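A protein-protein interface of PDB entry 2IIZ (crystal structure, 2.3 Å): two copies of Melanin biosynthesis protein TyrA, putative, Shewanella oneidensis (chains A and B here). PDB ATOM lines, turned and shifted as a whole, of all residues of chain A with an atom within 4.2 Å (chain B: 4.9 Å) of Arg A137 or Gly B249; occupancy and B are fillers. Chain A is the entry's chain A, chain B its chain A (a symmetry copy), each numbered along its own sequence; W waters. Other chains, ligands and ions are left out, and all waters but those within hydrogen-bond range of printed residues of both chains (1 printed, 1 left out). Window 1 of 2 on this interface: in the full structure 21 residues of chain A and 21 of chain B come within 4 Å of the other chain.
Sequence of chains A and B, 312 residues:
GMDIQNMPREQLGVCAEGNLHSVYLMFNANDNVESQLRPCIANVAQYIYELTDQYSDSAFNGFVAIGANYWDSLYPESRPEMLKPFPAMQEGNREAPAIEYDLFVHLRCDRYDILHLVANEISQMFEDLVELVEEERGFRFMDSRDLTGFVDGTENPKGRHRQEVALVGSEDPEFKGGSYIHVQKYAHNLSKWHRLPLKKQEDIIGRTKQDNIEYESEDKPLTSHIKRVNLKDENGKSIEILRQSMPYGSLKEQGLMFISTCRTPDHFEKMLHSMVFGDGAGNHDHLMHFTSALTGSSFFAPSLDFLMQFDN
Arg A137 touches Gly B249, and with the chains exchanged Gly A249 touches Arg B137. Of the 10 pairs that touch across the chains among the printed residues, 2 have their exchanged pair printed and touching as well.
Of the printed residues of chain B, His A116 touches Phe B139 (3.5 Å), Gly B249 (3.7 Å), Ser B250 (3.9 Å) and Gln B254 (2.5 Å). Of the printed residues of chain B, Glu A135 touches Ser B250 and Leu B251. Glu A136 touches none of the printed residues of chain B. Arg A137 touches two residues of chain B. Tyr A248 touches none of the printed residues of chain B. Of chain A, only His A116 (3.7 Å) and Arg A137 (3.95 Å) come within 4 Å of Gly B249. Of the printed residues of chain A, Gln B254 touches His A116. The nearest residue of chain B that does not touch Arg A137 is Leu B251 (4.5 Å).
The side-chain carboxylate of Glu A135 sits at hydrogen-bond distance from the side-chain hydroxyl of Ser B250. The side-chain amide oxygen (OE1) of Gln B254 sits at hydrogen-bond distance from a ring nitrogen (NE2) of His A116 (2.5 Å). N of Leu B251 is in hydrogen-bond range of OE1 of Glu A135 (3.0 Å).
NH2 of Arg A137 lies within salt-bridge range of OE2 of Glu A135 (3.0 Å). A ring nitrogen (ND1) of His A116 lies within hydrogen-bond range of the guanidinium group (NH1) of Arg A137 (3.0 Å). The backbone NH (N) of Phe B139 is in hydrogen-bond range of the backbone carbonyl oxygen (O) of Pro B247, at 2.9 Å. The side-chain hydroxyl (OH) of Tyr A112 lies within hydrogen-bond range of the guanidinium group (NH1) of Arg A137 (3.3 Å).
Water W1 lies within hydrogen-bond range of OH of Tyr A112 (2.5 Å), O of Gly B249 (2.8 Å) and O of Arg B137 (3.0 Å).
CG of Phe B139 touches CE1 of Tyr A112, 3.5 Å away. Phe B139 touches His A116 (CZ to ND1, 3.5 Å). CE1 of His A116 touches O of Gly B249 (3.7 Å). Ser B250 touches His A116 (N to CE1, 3.9 Å). O of Gly B249 touches NH1 of Arg A137 (3.95 Å). NH2 of Arg A137 touches CA of Ser B250 (3.8 Å). Gly A249 touches Arg B137 (O to NH1, 3.95 Å).
Of the 10 printed residues of chain B, 6 touch a printed residue of chain A. Printed residues of chain B that touch a printed residue of chain A: Arg B137, Phe B139, Gly B249, Ser B250, Leu B251 and Gln B254. Hydrophobic or aromatic side chains of chain B that line the printed part of chain A: Phe B139 and Leu B251. Along chain B the printed residues that touch a printed residue of chain A span positions 137 to 254. Of the 10 printed residues of chain A, 5 touch a printed residue of chain B. Hydrophobic or aromatic side chains of chain A within 4 Å of the printed part of chain B: Tyr A112 and His A116. Among the printed residues, 10 pairs touch across the chains.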
ATOM      1  N   SER A  22       0.977  21.225 -33.079  1.00  0.00           N
ATOM      2  CA  SER A  22       2.232  21.957 -33.153  1.00  0.00           C
ATOM      3  C   SER A  22       3.200  21.538 -32.049  1.00  0.00           C
ATOM      4  O   SER A  22       2.789  21.021 -31.003  1.00  0.00           O
ATOM      5  CB  SER A  22       1.950  23.448 -32.973  1.00  0.00           C
ATOM      6  OG  SER A  22       1.467  23.658 -31.666  1.00  0.00           O
ATOM      7  N   VAL A  23       4.490  21.790 -32.295  1.00  0.00           N
ATOM      8  CA  VAL A  23       5.558  21.570 -31.302  1.00  0.00           C
ATOM      9  C   VAL A  23       6.424  22.831 -31.205  1.00  0.00           C
ATOM     10  O   VAL A  23       6.747  23.485 -32.224  1.00  0.00           O
ATOM     11  CB  VAL A  23       6.426  20.400 -31.683  1.00  0.00           C
ATOM     12  CG1 VAL A  23       7.499  20.128 -30.634  1.00  0.00           C
ATOM     13  CG2 VAL A  23       5.555  19.151 -31.867  1.00  0.00           C
ATOM     14  N   TYR A 112       0.100  14.536 -35.684  1.00  0.00           N
ATOM     15  CA  TYR A 112       0.948  14.648 -34.500  1.00  0.00           C
ATOM     16  C   TYR A 112       2.099  13.694 -34.593  1.00  0.00           C
ATOM     17  O   TYR A 112       3.169  13.978 -34.103  1.00  0.00           O
ATOM     18  CB  TYR A 112       0.086  14.291 -33.302  1.00  0.00           C
ATOM     19  CG  TYR A 112       0.678  14.315 -31.911  1.00  0.00           C
ATOM     20  CD1 TYR A 112       1.446  13.245 -31.438  1.00  0.00           C
ATOM     21  CD2 TYR A 112       0.437  15.390 -31.048  1.00  0.00           C
ATOM     22  CE1 TYR A 112       1.972  13.256 -30.146  1.00  0.00           C
ATOM     23  CE2 TYR A 112       0.959  15.416 -29.740  1.00  0.00           C
ATOM     24  CZ  TYR A 112       1.728  14.345 -29.290  1.00  0.00           C
ATOM     25  OH  TYR A 112       2.263  14.338 -28.002  1.00  0.00           O
ATOM     26  N   HIS A 116       6.181  14.473 -34.087  1.00  0.00           N
ATOM     27  CA  HIS A 116       7.016  13.742 -33.158  1.00  0.00           C
ATOM     28  C   HIS A 116       8.257  13.314 -33.909  1.00  0.00           C
ATOM     29  O   HIS A 116       9.362  13.512 -33.438  1.00  0.00           O
ATOM     30  CB  HIS A 116       6.286  12.542 -32.599  1.00  0.00           C
ATOM     31  CG  HIS A 116       7.004  11.876 -31.471  1.00  0.00           C
ATOM     32  ND1 HIS A 116       6.836  12.254 -30.157  1.00  0.00           N
ATOM     33  CD2 HIS A 116       7.892  10.853 -31.463  1.00  0.00           C
ATOM     34  CE1 HIS A 116       7.592  11.491 -29.388  1.00  0.00           C
ATOM     35  NE2 HIS A 116       8.241  10.634 -30.155  1.00  0.00           N
ATOM     36  N   GLU A 135      10.089  22.196 -24.046  1.00  0.00           N
ATOM     37  CA  GLU A 135       9.288  21.621 -25.107  1.00  0.00           C
ATOM     38  C   GLU A 135       7.834  21.689 -24.693  1.00  0.00           C
ATOM     39  O   GLU A 135       7.494  21.370 -23.549  1.00  0.00           O
ATOM     40  CB  GLU A 135       9.670  20.171 -25.365  1.00  0.00           C
ATOM     41  CG  GLU A 135       8.662  19.477 -26.279  1.00  0.00           C
ATOM     42  CD  GLU A 135       9.092  18.104 -26.775  1.00  0.00           C
ATOM     43  OE1 GLU A 135      10.020  17.487 -26.170  1.00  0.00           O
ATOM     44  OE2 GLU A 135       8.478  17.655 -27.782  1.00  0.00           O
ATOM     45  N   GLU A 136       6.977  22.108 -25.617  1.00  0.00           N
ATOM     46  CA  GLU A 136       5.526  22.101 -25.388  1.00  0.00           C
ATOM     47  C   GLU A 136       4.830  21.695 -26.679  1.00  0.00           C
ATOM     48  O   GLU A 136       5.388  21.873 -27.766  1.00  0.00           O
ATOM     49  CB  GLU A 136       5.021  23.479 -24.938  1.00  0.00           C
ATOM     50  CG  GLU A 136       5.632  24.013 -23.630  1.00  0.00           C
ATOM     51  CD  GLU A 136       5.189  23.259 -22.371  1.00  0.00           C
ATOM     52  OE1 GLU A 136       4.235  22.461 -22.461  1.00  0.00           O
ATOM     53  OE2 GLU A 136       5.801  23.474 -21.291  1.00  0.00           O
ATOM     54  N   ARG A 137       3.617  21.157 -26.548  1.00  0.00           N
ATOM     55  CA  ARG A 137       2.810  20.739 -27.697  1.00  0.00           C
ATOM     56  C   ARG A 137       1.480  21.477 -27.697  1.00  0.00           C
ATOM     57  O   ARG A 137       0.748  21.467 -26.701  1.00  0.00           O
ATOM     58  CB  ARG A 137       2.616  19.207 -27.692  1.00  0.00           C
ATOM     59  CG  ARG A 137       3.983  18.487 -27.736  1.00  0.00           C
ATOM     60  CD  ARG A 137       4.029  17.086 -28.389  1.00  0.00           C
ATOM     61  NE  ARG A 137       5.438  16.703 -28.578  1.00  0.00           N
ATOM     62  CZ  ARG A 137       5.891  15.594 -29.173  1.00  0.00           C
ATOM     63  NH1 ARG A 137       5.053  14.680 -29.682  1.00  0.00           N
ATOM     64  NH2 ARG A 137       7.215  15.407 -29.255  1.00  0.00           N
ATOM     65  N   GLY A 138       1.195  22.120 -28.825  1.00  0.00           N
ATOM     66  CA  GLY A 138      -0.029  22.887 -29.030  1.00  0.00           C
ATOM     67  C   GLY A 138      -1.085  22.039 -29.715  1.00  0.00           C
ATOM     68  O   GLY A 138      -0.777  21.049 -30.411  1.00  0.00           O
ATOM     69  N   TYR A 248      -2.312  24.908 -25.345  1.00  0.00           N
ATOM     70  CA  TYR A 248      -1.231  23.984 -25.010  1.00  0.00           C
ATOM     71  C   TYR A 248      -1.404  23.417 -23.621  1.00  0.00           C
ATOM     72  O   TYR A 248      -2.177  23.938 -22.802  1.00  0.00           O
ATOM     73  CB  TYR A 248       0.124  24.697 -25.035  1.00  0.00           C
ATOM     74  CG  TYR A 248       0.470  25.301 -23.702  1.00  0.00           C
ATOM     75  CD1 TYR A 248       0.003  26.574 -23.341  1.00  0.00           C
ATOM     76  CD2 TYR A 248       1.249  24.609 -22.791  1.00  0.00           C
ATOM     77  CE1 TYR A 248       0.320  27.126 -22.110  1.00  0.00           C
ATOM     78  CE2 TYR A 248       1.564  25.156 -21.566  1.00  0.00           C
ATOM     79  CZ  TYR A 248       1.096  26.415 -21.232  1.00  0.00           C
ATOM     80  OH  TYR A 248       1.421  26.937 -20.004  1.00  0.00           O
ATOM     81  N   GLY A 249      -0.664  22.341 -23.360  1.00  0.00           N
ATOM     82  CA  GLY A 249      -0.457  21.869 -21.997  1.00  0.00           C
ATOM     83  C   GLY A 249      -1.316  20.693 -21.594  1.00  0.00           C
ATOM     84  O   GLY A 249      -1.654  19.842 -22.414  1.00  0.00           O
ATOM     85  N   GLU B 136       0.298  11.209 -18.811  1.00  0.00           N
ATOM     86  CA  GLU B 136       1.007  11.019 -20.084  1.00  0.00           C
ATOM     87  C   GLU B 136      -0.016  10.969 -21.209  1.00  0.00           C
ATOM     88  O   GLU B 136      -1.180  10.631 -20.974  1.00  0.00           O
ATOM     89  CB  GLU B 136       1.836   9.727 -20.079  1.00  0.00           C
ATOM     90  CG  GLU B 136       2.925   9.644 -18.996  1.00  0.00           C
ATOM     91  CD  GLU B 136       4.108  10.595 -19.215  1.00  0.00           C
ATOM     92  OE1 GLU B 136       4.214  11.167 -20.317  1.00  0.00           O
ATOM     93  OE2 GLU B 136       4.932  10.760 -18.276  1.00  0.00           O
ATOM     94  N   ARG B 137       0.428  11.304 -22.421  1.00  0.00           N
ATOM     95  CA  ARG B 137      -0.428  11.281 -23.610  1.00  0.00           C
ATOM     96  C   ARG B 137       0.157  10.346 -24.657  1.00  0.00           C
ATOM     97  O   ARG B 137       1.325  10.471 -25.039  1.00  0.00           O
ATOM     98  CB  ARG B 137      -0.624  12.710 -24.163  1.00  0.00           C
ATOM     99  CG  ARG B 137      -1.259  13.624 -23.090  1.00  0.00           C
ATOM    100  CD  ARG B 137      -2.121  14.808 -23.584  1.00  0.00           C
ATOM    101  NE  ARG B 137      -2.846  15.373 -22.434  1.00  0.00           N
ATOM    102  CZ  ARG B 137      -3.744  16.364 -22.464  1.00  0.00           C
ATOM    103  NH1 ARG B 137      -4.085  16.966 -23.613  1.00  0.00           N
ATOM    104  NH2 ARG B 137      -4.307  16.753 -21.312  1.00  0.00           N
ATOM    105  N   PHE B 139      -0.053   8.336 -28.497  1.00  0.00           N
ATOM    106  CA  PHE B 139      -0.417   8.641 -29.865  1.00  0.00           C
ATOM    107  C   PHE B 139      -0.099   7.478 -30.796  1.00  0.00           C
ATOM    108  O   PHE B 139       0.921   6.815 -30.623  1.00  0.00           O
ATOM    109  CB  PHE B 139       0.308   9.890 -30.321  1.00  0.00           C
ATOM    110  CG  PHE B 139       1.805   9.767 -30.307  1.00  0.00           C
ATOM    111  CD1 PHE B 139       2.521   9.950 -29.134  1.00  0.00           C
ATOM    112  CD2 PHE B 139       2.499   9.476 -31.472  1.00  0.00           C
ATOM    113  CE1 PHE B 139       3.910   9.842 -29.116  1.00  0.00           C
ATOM    114  CE2 PHE B 139       3.898   9.369 -31.465  1.00  0.00           C
ATOM    115  CZ  PHE B 139       4.598   9.554 -30.285  1.00  0.00           C
ATOM    116  N   PRO B 247       2.419   4.378 -28.379  1.00  0.00           N
ATOM    117  CA  PRO B 247       3.591   5.231 -28.185  1.00  0.00           C
ATOM    118  C   PRO B 247       3.232   6.394 -27.280  1.00  0.00           C
ATOM    119  O   PRO B 247       2.058   6.737 -27.201  1.00  0.00           O
ATOM    120  CB  PRO B 247       3.886   5.761 -29.608  1.00  0.00           C
ATOM    121  CG  PRO B 247       3.329   4.712 -30.497  1.00  0.00           C
ATOM    122  CD  PRO B 247       2.083   4.248 -29.804  1.00  0.00           C
ATOM    123  N   TYR B 248       4.227   6.989 -26.618  1.00  0.00           N
ATOM    124  CA  TYR B 248       4.004   8.140 -25.746  1.00  0.00           C
ATOM    125  C   TYR B 248       5.247   8.991 -25.632  1.00  0.00           C
ATOM    126  O   TYR B 248       6.359   8.559 -25.975  1.00  0.00           O
ATOM    127  CB  TYR B 248       3.639   7.689 -24.330  1.00  0.00           C
ATOM    128  CG  TYR B 248       4.857   7.500 -23.466  1.00  0.00           C
ATOM    129  CD1 TYR B 248       5.572   6.293 -23.478  1.00  0.00           C
ATOM    130  CD2 TYR B 248       5.308   8.518 -22.645  1.00  0.00           C
ATOM    131  CE1 TYR B 248       6.695   6.122 -22.685  1.00  0.00           C
ATOM    132  CE2 TYR B 248       6.427   8.351 -21.856  1.00  0.00           C
ATOM    133  CZ  TYR B 248       7.115   7.150 -21.881  1.00  0.00           C
ATOM    134  OH  TYR B 248       8.227   7.009 -21.088  1.00  0.00           O
ATOM    135  N   GLY B 249       5.047  10.209 -25.135  1.00  0.00           N
ATOM    136  CA  GLY B 249       6.150  11.029 -24.654  1.00  0.00           C
ATOM    137  C   GLY B 249       6.613  12.100 -25.615  1.00  0.00           C
ATOM    138  O   GLY B 249       5.825  12.652 -26.379  1.00  0.00           O
ATOM    139  N   SER B 250       7.916  12.382 -25.567  1.00  0.00           N
ATOM    140  CA  SER B 250       8.484  13.598 -26.130  1.00  0.00           C
ATOM    141  C   SER B 250       9.999  13.488 -26.119  1.00  0.00           C
ATOM    142  O   SER B 250      10.537  12.436 -25.796  1.00  0.00           O
ATOM    143  CB  SER B 250       8.089  14.777 -25.264  1.00  0.00           C
ATOM    144  OG  SER B 250       8.986  14.877 -24.172  1.00  0.00           O
ATOM    145  N   LEU B 251      10.690  14.569 -26.461  1.00  0.00           N
ATOM    146  CA  LEU B 251      12.144  14.499 -26.605  1.00  0.00           C
ATOM    147  C   LEU B 251      12.804  14.079 -25.299  1.00  0.00           C
ATOM    148  O   LEU B 251      13.598  13.155 -25.306  1.00  0.00           O
ATOM    149  CB  LEU B 251      12.757  15.820 -27.116  1.00  0.00           C
ATOM    150  CG  LEU B 251      12.488  16.280 -28.566  1.00  0.00           C
ATOM    151  CD1 LEU B 251      13.294  17.523 -28.899  1.00  0.00           C
ATOM    152  CD2 LEU B 251      12.807  15.199 -29.582  1.00  0.00           C
ATOM    153  N   GLU B 253      11.787  12.235 -22.932  1.00  0.00           N
ATOM    154  CA  GLU B 253      11.577  10.793 -22.708  1.00  0.00           C
ATOM    155  C   GLU B 253      10.416  10.294 -23.567  1.00  0.00           C
ATOM    156  O   GLU B 253       9.372  10.961 -23.684  1.00  0.00           O
ATOM    157  CB  GLU B 253      11.310  10.570 -21.206  1.00  0.00           C
ATOM    158  CG  GLU B 253      10.806   9.202 -20.758  1.00  0.00           C
ATOM    159  CD  GLU B 253      10.284   9.242 -19.312  1.00  0.00           C
ATOM    160  OE1 GLU B 253      11.080   9.503 -18.393  1.00  0.00           O
ATOM    161  OE2 GLU B 253       9.077   9.014 -19.094  1.00  0.00           O
ATOM    162  N   GLN B 254      10.606   9.120 -24.171  1.00  0.00           N
ATOM    163  CA  GLN B 254       9.644   8.576 -25.112  1.00  0.00           C
ATOM    164  C   GLN B 254       9.778   7.071 -25.315  1.00  0.00           C
ATOM    165  O   GLN B 254      10.880   6.512 -25.328  1.00  0.00           O
ATOM    166  CB  GLN B 254       9.800   9.265 -26.453  1.00  0.00           C
ATOM    167  CG  GLN B 254      11.068   8.918 -27.225  1.00  0.00           C
ATOM    168  CD  GLN B 254      11.216   9.824 -28.427  1.00  0.00           C
ATOM    169  OE1 GLN B 254      10.472   9.713 -29.378  1.00  0.00           O
ATOM    170  NE2 GLN B 254      12.171  10.720 -28.381  1.00  0.00           N
HETATM  171  O   HOH W   1       3.009  12.379 -26.641  1.00  0.00           O
